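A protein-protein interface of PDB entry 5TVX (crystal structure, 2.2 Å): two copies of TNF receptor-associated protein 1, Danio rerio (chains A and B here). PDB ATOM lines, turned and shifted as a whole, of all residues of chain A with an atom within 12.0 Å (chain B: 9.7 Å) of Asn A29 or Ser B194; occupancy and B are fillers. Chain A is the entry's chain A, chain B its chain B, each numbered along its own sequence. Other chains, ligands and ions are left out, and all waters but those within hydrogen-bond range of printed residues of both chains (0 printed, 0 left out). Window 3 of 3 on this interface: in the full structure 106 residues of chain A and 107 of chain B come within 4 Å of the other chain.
The side-chain amino group (NZ) of Lys B201 lies within salt-bridge range of the side-chain carboxylate (OE1) of Glu A28 (2.9 Å). The backbone carbonyl oxygen (O) of Gly B195 lies within hydrogen-bond range of the side-chain hydroxyl (OG1) of Thr A27 (2.9 Å). O of Glu B192 lies within hydrogen-bond range of N of Gln A31, 3.1 Å away. The side-chain amino group (NZ) of Lys B201 sits at hydrogen-bond distance from the backbone carbonyl oxygen (O) of Thr A25, at 2.8 Å. The backbone carbonyl oxygen (O) of Asn A29 is in hydrogen-bond range of the backbone NH (N) of Ser B194 (3.3 Å).
The backbone carbonyl oxygen (O) of Ala B191 lies within hydrogen-bond range of the backbone NH (N) of Lys B179. The backbone carbonyl oxygen (O) of Ala B193 sits close to the backbone NH (N) of Gly B177 (3.2 Å). The side-chain amide nitrogen (NE2) of Gln B169 is in hydrogen-bond range of the backbone carbonyl oxygen (O) of Val B196. The backbone carbonyl oxygen of Tyr B167 is in hydrogen-bond range of the backbone NH of Lys B201 (2.7 Å).
Among the printed residues, merely in contact across the chains: Ile A23 with Arg B197, Thr A27 with Ser B194, Glu A28 with Tyr B167, Glu A28 with Ser B194, Glu A28 with Gly B195, Glu A28 with Val B196, Asn A29 with Ala B193, Val A30 with Lys B179, Val A30 with Ala B191, Val A30 with Glu B192, Ser A33 with Ala B191 and Phe A34 with Ala B191.
Asn A29 touches two residues of chain B. Val A30 touches just these residues of chain B: Lys B179 (3.7 Å), Ala B191 (3.6 Å) and Glu B192 (3.6 Å). Of the printed residues of chain A, Tyr B167 touches Glu A28 (3.6 Å). No residue of chain A comes within 4 Å of Gly B177. Tyr B178 touches none of the printed residues of chain A. Printed residues of chain A within 4 Å of Lys B179: Val A30 (3.7 Å). Of chain A, only Thr A27, Glu A28 and Asn A29 come within 4 Å of Ser B194. Gly B195 touches just these residues of chain A: Thr A27 and Glu A28. The nearest residue of chain B that does not touch Asn A29 is Glu B192 (4.4 Å). The nearest printed residue of chain A that does not touch Lys B201 is Asp A26 (4.6 Å).
Hydrophobic or aromatic side chains of chain A within 4 Å of the printed part of chain B: Ile A23, Val A30 and Phe A34. Of the 17 printed residues of chain B, 10 touch a printed residue of chain A.
No position is printed for both chains. Of the 17 pairs that touch across the chains among the printed residues, none has its exchanged pair printed and touching as well.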
ATOM      1  N   ILE A  23      20.445  13.635 -25.589  1.00  0.00           N
ATOM      2  CA  ILE A  23      19.143  14.240 -25.351  1.00  0.00           C
ATOM      3  C   ILE A  23      18.075  13.210 -25.030  1.00  0.00           C
ATOM      4  O   ILE A  23      16.904  13.588 -24.829  1.00  0.00           O
ATOM      5  CB  ILE A  23      18.702  15.091 -26.554  1.00  0.00           C
ATOM      6  CG1 ILE A  23      18.260  14.181 -27.706  1.00  0.00           C
ATOM      7  CG2 ILE A  23      19.840  15.985 -27.011  1.00  0.00           C
ATOM      8  CD1 ILE A  23      17.593  14.924 -28.857  1.00  0.00           C
ATOM      9  N   THR A  25      16.085  10.972 -22.769  1.00  0.00           N
ATOM     10  CA  THR A  25      15.819  10.954 -21.335  1.00  0.00           C
ATOM     11  C   THR A  25      14.456  10.331 -21.069  1.00  0.00           C
ATOM     12  O   THR A  25      13.552  10.399 -21.906  1.00  0.00           O
ATOM     13  CB  THR A  25      15.853  12.369 -20.725  1.00  0.00           C
ATOM     14  OG1 THR A  25      14.948  13.227 -21.439  1.00  0.00           O
ATOM     15  CG2 THR A  25      17.257  12.946 -20.777  1.00  0.00           C
ATOM     16  N   ASP A  26      14.313   9.739 -19.880  1.00  0.00           N
ATOM     17  CA  ASP A  26      13.054   9.134 -19.440  1.00  0.00           C
ATOM     18  C   ASP A  26      12.186  10.223 -18.821  1.00  0.00           C
ATOM     19  O   ASP A  26      12.177  10.430 -17.607  1.00  0.00           O
ATOM     20  CB  ASP A  26      13.314   7.998 -18.456  1.00  0.00           C
ATOM     21  CG  ASP A  26      12.122   7.053 -18.319  1.00  0.00           C
ATOM     22  OD1 ASP A  26      10.963   7.502 -18.474  1.00  0.00           O
ATOM     23  OD2 ASP A  26      12.348   5.853 -18.059  1.00  0.00           O
ATOM     24  N   THR A  27      11.426  10.913 -19.667  1.00  0.00           N
ATOM     25  CA  THR A  27      10.632  12.052 -19.241  1.00  0.00           C
ATOM     26  C   THR A  27       9.157  11.913 -19.565  1.00  0.00           C
ATOM     27  O   THR A  27       8.356  12.735 -19.095  1.00  0.00           O
ATOM     28  CB  THR A  27      11.157  13.350 -19.888  1.00  0.00           C
ATOM     29  OG1 THR A  27      11.176  13.211 -21.315  1.00  0.00           O
ATOM     30  CG2 THR A  27      12.563  13.673 -19.398  1.00  0.00           C
ATOM     31  N   GLU A  28       8.771  10.910 -20.341  1.00  0.00           N
ATOM     32  CA  GLU A  28       7.402  10.773 -20.807  1.00  0.00           C
ATOM     33  C   GLU A  28       6.603   9.900 -19.851  1.00  0.00           C
ATOM     34  O   GLU A  28       7.100   8.884 -19.351  1.00  0.00           O
ATOM     35  CB  GLU A  28       7.370  10.170 -22.215  1.00  0.00           C
ATOM     36  CG  GLU A  28       8.266  10.862 -23.230  1.00  0.00           C
ATOM     37  CD  GLU A  28       9.703  10.361 -23.181  1.00  0.00           C
ATOM     38  OE1 GLU A  28      10.549  10.903 -23.918  1.00  0.00           O
ATOM     39  OE2 GLU A  28       9.992   9.428 -22.402  1.00  0.00           O
ATOM     40  N   ASN A  29       5.363  10.310 -19.598  1.00  0.00           N
ATOM     41  CA  ASN A  29       4.429   9.533 -18.798  1.00  0.00           C
ATOM     42  C   ASN A  29       3.074   9.608 -19.477  1.00  0.00           C
ATOM     43  O   ASN A  29       2.662  10.685 -19.919  1.00  0.00           O
ATOM     44  CB  ASN A  29       4.350  10.052 -17.353  1.00  0.00           C
ATOM     45  CG  ASN A  29       5.601   9.719 -16.532  1.00  0.00           C
ATOM     46  OD1 ASN A  29       5.979   8.551 -16.384  1.00  0.00           O
ATOM     47  ND2 ASN A  29       6.249  10.753 -16.003  1.00  0.00           N
ATOM     48  N   VAL A  30       2.403   8.460 -19.584  1.00  0.00           N
ATOM     49  CA  VAL A  30       1.096   8.412 -20.229  1.00  0.00           C
ATOM     50  C   VAL A  30       0.065   9.058 -19.320  1.00  0.00           C
ATOM     51  O   VAL A  30      -0.070   8.691 -18.146  1.00  0.00           O
ATOM     52  CB  VAL A  30       0.702   6.964 -20.555  1.00  0.00           C
ATOM     53  CG1 VAL A  30      -0.793   6.877 -20.869  1.00  0.00           C
ATOM     54  CG2 VAL A  30       1.537   6.429 -21.713  1.00  0.00           C
ATOM     55  N   GLN A  31      -0.670  10.025 -19.856  1.00  0.00           N
ATOM     56  CA  GLN A  31      -1.805  10.600 -19.152  1.00  0.00           C
ATOM     57  C   GLN A  31      -2.984  10.626 -20.109  1.00  0.00           C
ATOM     58  O   GLN A  31      -2.915  11.254 -21.169  1.00  0.00           O
ATOM     59  CB  GLN A  31      -1.487  11.996 -18.608  1.00  0.00           C
ATOM     60  CG  GLN A  31      -0.915  11.965 -17.186  1.00  0.00           C
ATOM     61  CD  GLN A  31      -1.738  11.088 -16.242  1.00  0.00           C
ATOM     62  OE1 GLN A  31      -1.332   9.976 -15.894  1.00  0.00           O
ATOM     63  NE2 GLN A  31      -2.901  11.587 -15.829  1.00  0.00           N
ATOM     64  N   GLY A  32      -4.056   9.935 -19.735  1.00  0.00           N
ATOM     65  CA  GLY A  32      -5.214   9.734 -20.572  1.00  0.00           C
ATOM     66  C   GLY A  32      -5.506   8.257 -20.686  1.00  0.00           C
ATOM     67  O   GLY A  32      -5.051   7.449 -19.868  1.00  0.00           O
ATOM     68  N   SER A  33      -6.270   7.902 -21.714  1.00  0.00           N
ATOM     69  CA  SER A  33      -6.661   6.523 -21.964  1.00  0.00           C
ATOM     70  C   SER A  33      -6.017   6.012 -23.248  1.00  0.00           C
ATOM     71  O   SER A  33      -5.423   6.768 -24.023  1.00  0.00           O
ATOM     72  CB  SER A  33      -8.191   6.393 -22.044  1.00  0.00           C
ATOM     73  OG  SER A  33      -8.790   6.446 -20.757  1.00  0.00           O
ATOM     74  N   PHE A  34      -6.131   4.703 -23.452  1.00  0.00           N
ATOM     75  CA  PHE A  34      -5.745   4.084 -24.712  1.00  0.00           C
ATOM     76  C   PHE A  34      -6.863   4.222 -25.735  1.00  0.00           C
ATOM     77  O   PHE A  34      -8.043   4.045 -25.412  1.00  0.00           O
ATOM     78  CB  PHE A  34      -5.446   2.598 -24.516  1.00  0.00           C
ATOM     79  CG  PHE A  34      -4.213   2.321 -23.712  1.00  0.00           C
ATOM     80  CD1 PHE A  34      -3.149   3.214 -23.707  1.00  0.00           C
ATOM     81  CD2 PHE A  34      -4.115   1.149 -22.966  1.00  0.00           C
ATOM     82  CE1 PHE A  34      -2.008   2.948 -22.967  1.00  0.00           C
ATOM     83  CE2 PHE A  34      -2.980   0.874 -22.223  1.00  0.00           C
ATOM     84  CZ  PHE A  34      -1.924   1.776 -22.222  1.00  0.00           C
ATOM     85  N   TYR B 167       7.230   7.944 -29.140  1.00  0.00           N
ATOM     86  CA  TYR B 167       6.824   9.180 -28.479  1.00  0.00           C
ATOM     87  C   TYR B 167       7.040  10.301 -29.474  1.00  0.00           C
ATOM     88  O   TYR B 167       8.163  10.501 -29.946  1.00  0.00           O
ATOM     89  CB  TYR B 167       7.638   9.443 -27.207  1.00  0.00           C
ATOM     90  CG  TYR B 167       7.656   8.277 -26.238  1.00  0.00           C
ATOM     91  CD1 TYR B 167       8.583   7.255 -26.383  1.00  0.00           C
ATOM     92  CD2 TYR B 167       6.747   8.195 -25.184  1.00  0.00           C
ATOM     93  CE1 TYR B 167       8.610   6.183 -25.516  1.00  0.00           C
ATOM     94  CE2 TYR B 167       6.762   7.115 -24.300  1.00  0.00           C
ATOM     95  CZ  TYR B 167       7.698   6.109 -24.474  1.00  0.00           C
ATOM     96  OH  TYR B 167       7.742   5.020 -23.631  1.00  0.00           O
ATOM     97  N   SER B 168       5.977  11.015 -29.812  1.00  0.00           N
ATOM     98  CA  SER B 168       6.093  12.007 -30.866  1.00  0.00           C
ATOM     99  C   SER B 168       5.404  13.298 -30.453  1.00  0.00           C
ATOM    100  O   SER B 168       4.402  13.279 -29.732  1.00  0.00           O
ATOM    101  CB  SER B 168       5.512  11.490 -32.184  1.00  0.00           C
ATOM    102  OG  SER B 168       5.979  12.287 -33.250  1.00  0.00           O
ATOM    103  N   GLN B 169       5.961  14.420 -30.923  1.00  0.00           N
ATOM    104  CA  GLN B 169       5.466  15.760 -30.601  1.00  0.00           C
ATOM    105  C   GLN B 169       5.483  16.617 -31.857  1.00  0.00           C
ATOM    106  O   GLN B 169       6.554  16.916 -32.393  1.00  0.00           O
ATOM    107  CB  GLN B 169       6.304  16.425 -29.506  1.00  0.00           C
ATOM    108  CG  GLN B 169       5.918  17.874 -29.228  1.00  0.00           C
ATOM    109  CD  GLN B 169       4.593  18.000 -28.495  1.00  0.00           C
ATOM    110  OE1 GLN B 169       3.561  18.288 -29.102  1.00  0.00           O
ATOM    111  NE2 GLN B 169       4.619  17.785 -27.179  1.00  0.00           N
ATOM    112  N   ALA B 175      -0.746  21.374 -29.327  1.00  0.00           N
ATOM    113  CA  ALA B 175      -0.314  20.000 -29.678  1.00  0.00           C
ATOM    114  C   ALA B 175       0.054  19.188 -28.443  1.00  0.00           C
ATOM    115  O   ALA B 175       0.948  19.566 -27.684  1.00  0.00           O
ATOM    116  CB  ALA B 175       0.860  20.014 -30.628  1.00  0.00           C
ATOM    117  N   PRO B 176      -0.635  18.074 -28.244  1.00  0.00           N
ATOM    118  CA  PRO B 176      -0.290  17.163 -27.153  1.00  0.00           C
ATOM    119  C   PRO B 176       0.809  16.198 -27.586  1.00  0.00           C
ATOM    120  O   PRO B 176       1.189  16.122 -28.754  1.00  0.00           O
ATOM    121  CB  PRO B 176      -1.603  16.413 -26.883  1.00  0.00           C
ATOM    122  CG  PRO B 176      -2.645  17.040 -27.808  1.00  0.00           C
ATOM    123  CD  PRO B 176      -1.875  17.674 -28.918  1.00  0.00           C
ATOM    124  N   GLY B 177       1.320  15.462 -26.608  1.00  0.00           N
ATOM    125  CA  GLY B 177       2.275  14.404 -26.858  1.00  0.00           C
ATOM    126  C   GLY B 177       1.571  13.060 -26.840  1.00  0.00           C
ATOM    127  O   GLY B 177       0.613  12.852 -26.094  1.00  0.00           O
ATOM    128  N   TYR B 178       2.039  12.140 -27.676  1.00  0.00           N
ATOM    129  CA  TYR B 178       1.390  10.845 -27.757  1.00  0.00           C
ATOM    130  C   TYR B 178       2.420   9.730 -27.671  1.00  0.00           C
ATOM    131  O   TYR B 178       3.588   9.909 -28.025  1.00  0.00           O
ATOM    132  CB  TYR B 178       0.557  10.725 -29.037  1.00  0.00           C
ATOM    133  CG  TYR B 178      -0.599  11.693 -29.074  1.00  0.00           C
ATOM    134  CD1 TYR B 178      -1.810  11.370 -28.476  1.00  0.00           C
ATOM    135  CD2 TYR B 178      -0.475  12.942 -29.677  1.00  0.00           C
ATOM    136  CE1 TYR B 178      -2.868  12.247 -28.488  1.00  0.00           C
ATOM    137  CE2 TYR B 178      -1.542  13.836 -29.691  1.00  0.00           C
ATOM    138  CZ  TYR B 178      -2.733  13.476 -29.096  1.00  0.00           C
ATOM    139  OH  TYR B 178      -3.806  14.335 -29.092  1.00  0.00           O
ATOM    140  N   LYS B 179       1.977   8.582 -27.166  1.00  0.00           N
ATOM    141  CA  LYS B 179       2.784   7.372 -27.142  1.00  0.00           C
ATOM    142  C   LYS B 179       2.078   6.309 -27.965  1.00  0.00           C
ATOM    143  O   LYS B 179       0.943   5.924 -27.661  1.00  0.00           O
ATOM    144  CB  LYS B 179       3.027   6.884 -25.719  1.00  0.00           C
ATOM    145  CG  LYS B 179       3.836   5.599 -25.650  1.00  0.00           C
ATOM    146  CD  LYS B 179       3.811   5.010 -24.223  1.00  0.00           C
ATOM    147  CE  LYS B 179       4.604   3.713 -24.160  1.00  0.00           C
ATOM    148  NZ  LYS B 179       4.538   3.014 -22.855  1.00  0.00           N
ATOM    149  N   ALA B 191      -1.920   6.643 -26.744  1.00  0.00           N
ATOM    150  CA  ALA B 191      -2.316   7.335 -25.527  1.00  0.00           C
ATOM    151  C   ALA B 191      -1.628   8.690 -25.471  1.00  0.00           C
ATOM    152  O   ALA B 191      -0.484   8.832 -25.912  1.00  0.00           O
ATOM    153  CB  ALA B 191      -1.962   6.515 -24.284  1.00  0.00           C
ATOM    154  N   GLU B 192      -2.330   9.686 -24.943  1.00  0.00           N
ATOM    155  CA  GLU B 192      -1.738  11.007 -24.784  1.00  0.00           C
ATOM    156  C   GLU B 192      -0.565  10.936 -23.811  1.00  0.00           C
ATOM    157  O   GLU B 192      -0.488  10.045 -22.963  1.00  0.00           O
ATOM    158  CB  GLU B 192      -2.796  11.993 -24.297  1.00  0.00           C
ATOM    159  CG  GLU B 192      -2.509  13.444 -24.633  1.00  0.00           C
ATOM    160  CD  GLU B 192      -3.638  14.375 -24.209  1.00  0.00           C
ATOM    161  OE1 GLU B 192      -4.756  13.880 -23.950  1.00  0.00           O
ATOM    162  OE2 GLU B 192      -3.405  15.599 -24.128  1.00  0.00           O
ATOM    163  N   ALA B 193       0.374  11.868 -23.951  1.00  0.00           N
ATOM    164  CA  ALA B 193       1.579  11.828 -23.134  1.00  0.00           C
ATOM    165  C   ALA B 193       2.148  13.228 -22.953  1.00  0.00           C
ATOM    166  O   ALA B 193       2.038  14.084 -23.834  1.00  0.00           O
ATOM    167  CB  ALA B 193       2.651  10.913 -23.746  1.00  0.00           C
ATOM    168  N   SER B 194       2.768  13.442 -21.798  1.00  0.00           N
ATOM    169  CA  SER B 194       3.483  14.669 -21.483  1.00  0.00           C
ATOM    170  C   SER B 194       4.983  14.398 -21.475  1.00  0.00           C
ATOM    171  O   SER B 194       5.434  13.250 -21.524  1.00  0.00           O
ATOM    172  CB  SER B 194       3.025  15.242 -20.132  1.00  0.00           C
ATOM    173  OG  SER B 194       3.132  14.284 -19.088  1.00  0.00           O
ATOM    174  N   GLY B 195       5.761  15.474 -21.405  1.00  0.00           N
ATOM    175  CA  GLY B 195       7.204  15.333 -21.432  1.00  0.00           C
ATOM    176  C   GLY B 195       7.776  14.844 -22.746  1.00  0.00           C
ATOM    177  O   GLY B 195       8.883  14.291 -22.765  1.00  0.00           O
ATOM    178  N   VAL B 196       7.060  15.028 -23.852  1.00  0.00           N
ATOM    179  CA  VAL B 196       7.537  14.588 -25.157  1.00  0.00           C
ATOM    180  C   VAL B 196       8.197  15.767 -25.854  1.00  0.00           C
ATOM    181  O   VAL B 196       7.557  16.795 -26.106  1.00  0.00           O
ATOM    182  CB  VAL B 196       6.410  13.987 -26.008  1.00  0.00           C
ATOM    183  CG1 VAL B 196       6.952  13.611 -27.374  1.00  0.00           C
ATOM    184  CG2 VAL B 196       5.866  12.757 -25.314  1.00  0.00           C
ATOM    185  N   ARG B 197       9.481  15.606 -26.155  1.00  0.00           N
ATOM    186  CA  ARG B 197      10.258  16.633 -26.821  1.00  0.00           C
ATOM    187  C   ARG B 197       9.903  16.696 -28.301  1.00  0.00           C
ATOM    188  O   ARG B 197       9.662  15.664 -28.945  1.00  0.00           O
ATOM    189  CB  ARG B 197      11.746  16.345 -26.641  1.00  0.00           C
ATOM    190  CG  ARG B 197      12.688  17.430 -27.135  1.00  0.00           C
ATOM    191  CD  ARG B 197      14.086  16.862 -27.234  1.00  0.00           C
ATOM    192  NE  ARG B 197      15.051  17.810 -27.767  1.00  0.00           N
ATOM    193  CZ  ARG B 197      15.933  18.465 -27.022  1.00  0.00           C
ATOM    194  NH1 ARG B 197      15.961  18.276 -25.702  1.00  0.00           N
ATOM    195  NH2 ARG B 197      16.782  19.307 -27.599  1.00  0.00           N
ATOM    196  N   GLN B 198       9.832  17.922 -28.817  1.00  0.00           N
ATOM    197  CA  GLN B 198       9.705  18.186 -30.242  1.00  0.00           C
ATOM    198  C   GLN B 198      10.469  17.159 -31.069  1.00  0.00           C
ATOM    199  O   GLN B 198      11.677  16.982 -30.899  1.00  0.00           O
ATOM    200  CB  GLN B 198      10.232  19.589 -30.542  1.00  0.00           C
ATOM    201  CG  GLN B 198      10.179  19.943 -32.015  1.00  0.00           C
ATOM    202  CD  GLN B 198       8.779  20.278 -32.469  1.00  0.00           C
ATOM    203  OE1 GLN B 198       8.122  19.485 -33.139  1.00  0.00           O
ATOM    204  NE2 GLN B 198       8.312  21.464 -32.103  1.00  0.00           N
ATOM    205  N   LYS B 201      10.734   9.933 -30.674  1.00  0.00           N
ATOM    206  CA  LYS B 201      11.614   8.960 -30.034  1.00  0.00           C
ATOM    207  C   LYS B 201      11.018   7.566 -30.185  1.00  0.00           C
ATOM    208  O   LYS B 201       9.840   7.358 -29.875  1.00  0.00           O
ATOM    209  CB  LYS B 201      11.811   9.275 -28.557  1.00  0.00           C
ATOM    210  CG  LYS B 201      12.631   8.242 -27.826  1.00  0.00           C
ATOM    211  CD  LYS B 201      13.107   8.773 -26.481  1.00  0.00           C
ATOM    212  CE  LYS B 201      12.090   8.507 -25.378  1.00  0.00           C
ATOM    213  NZ  LYS B 201      12.630   8.824 -24.019  1.00  0.00           N
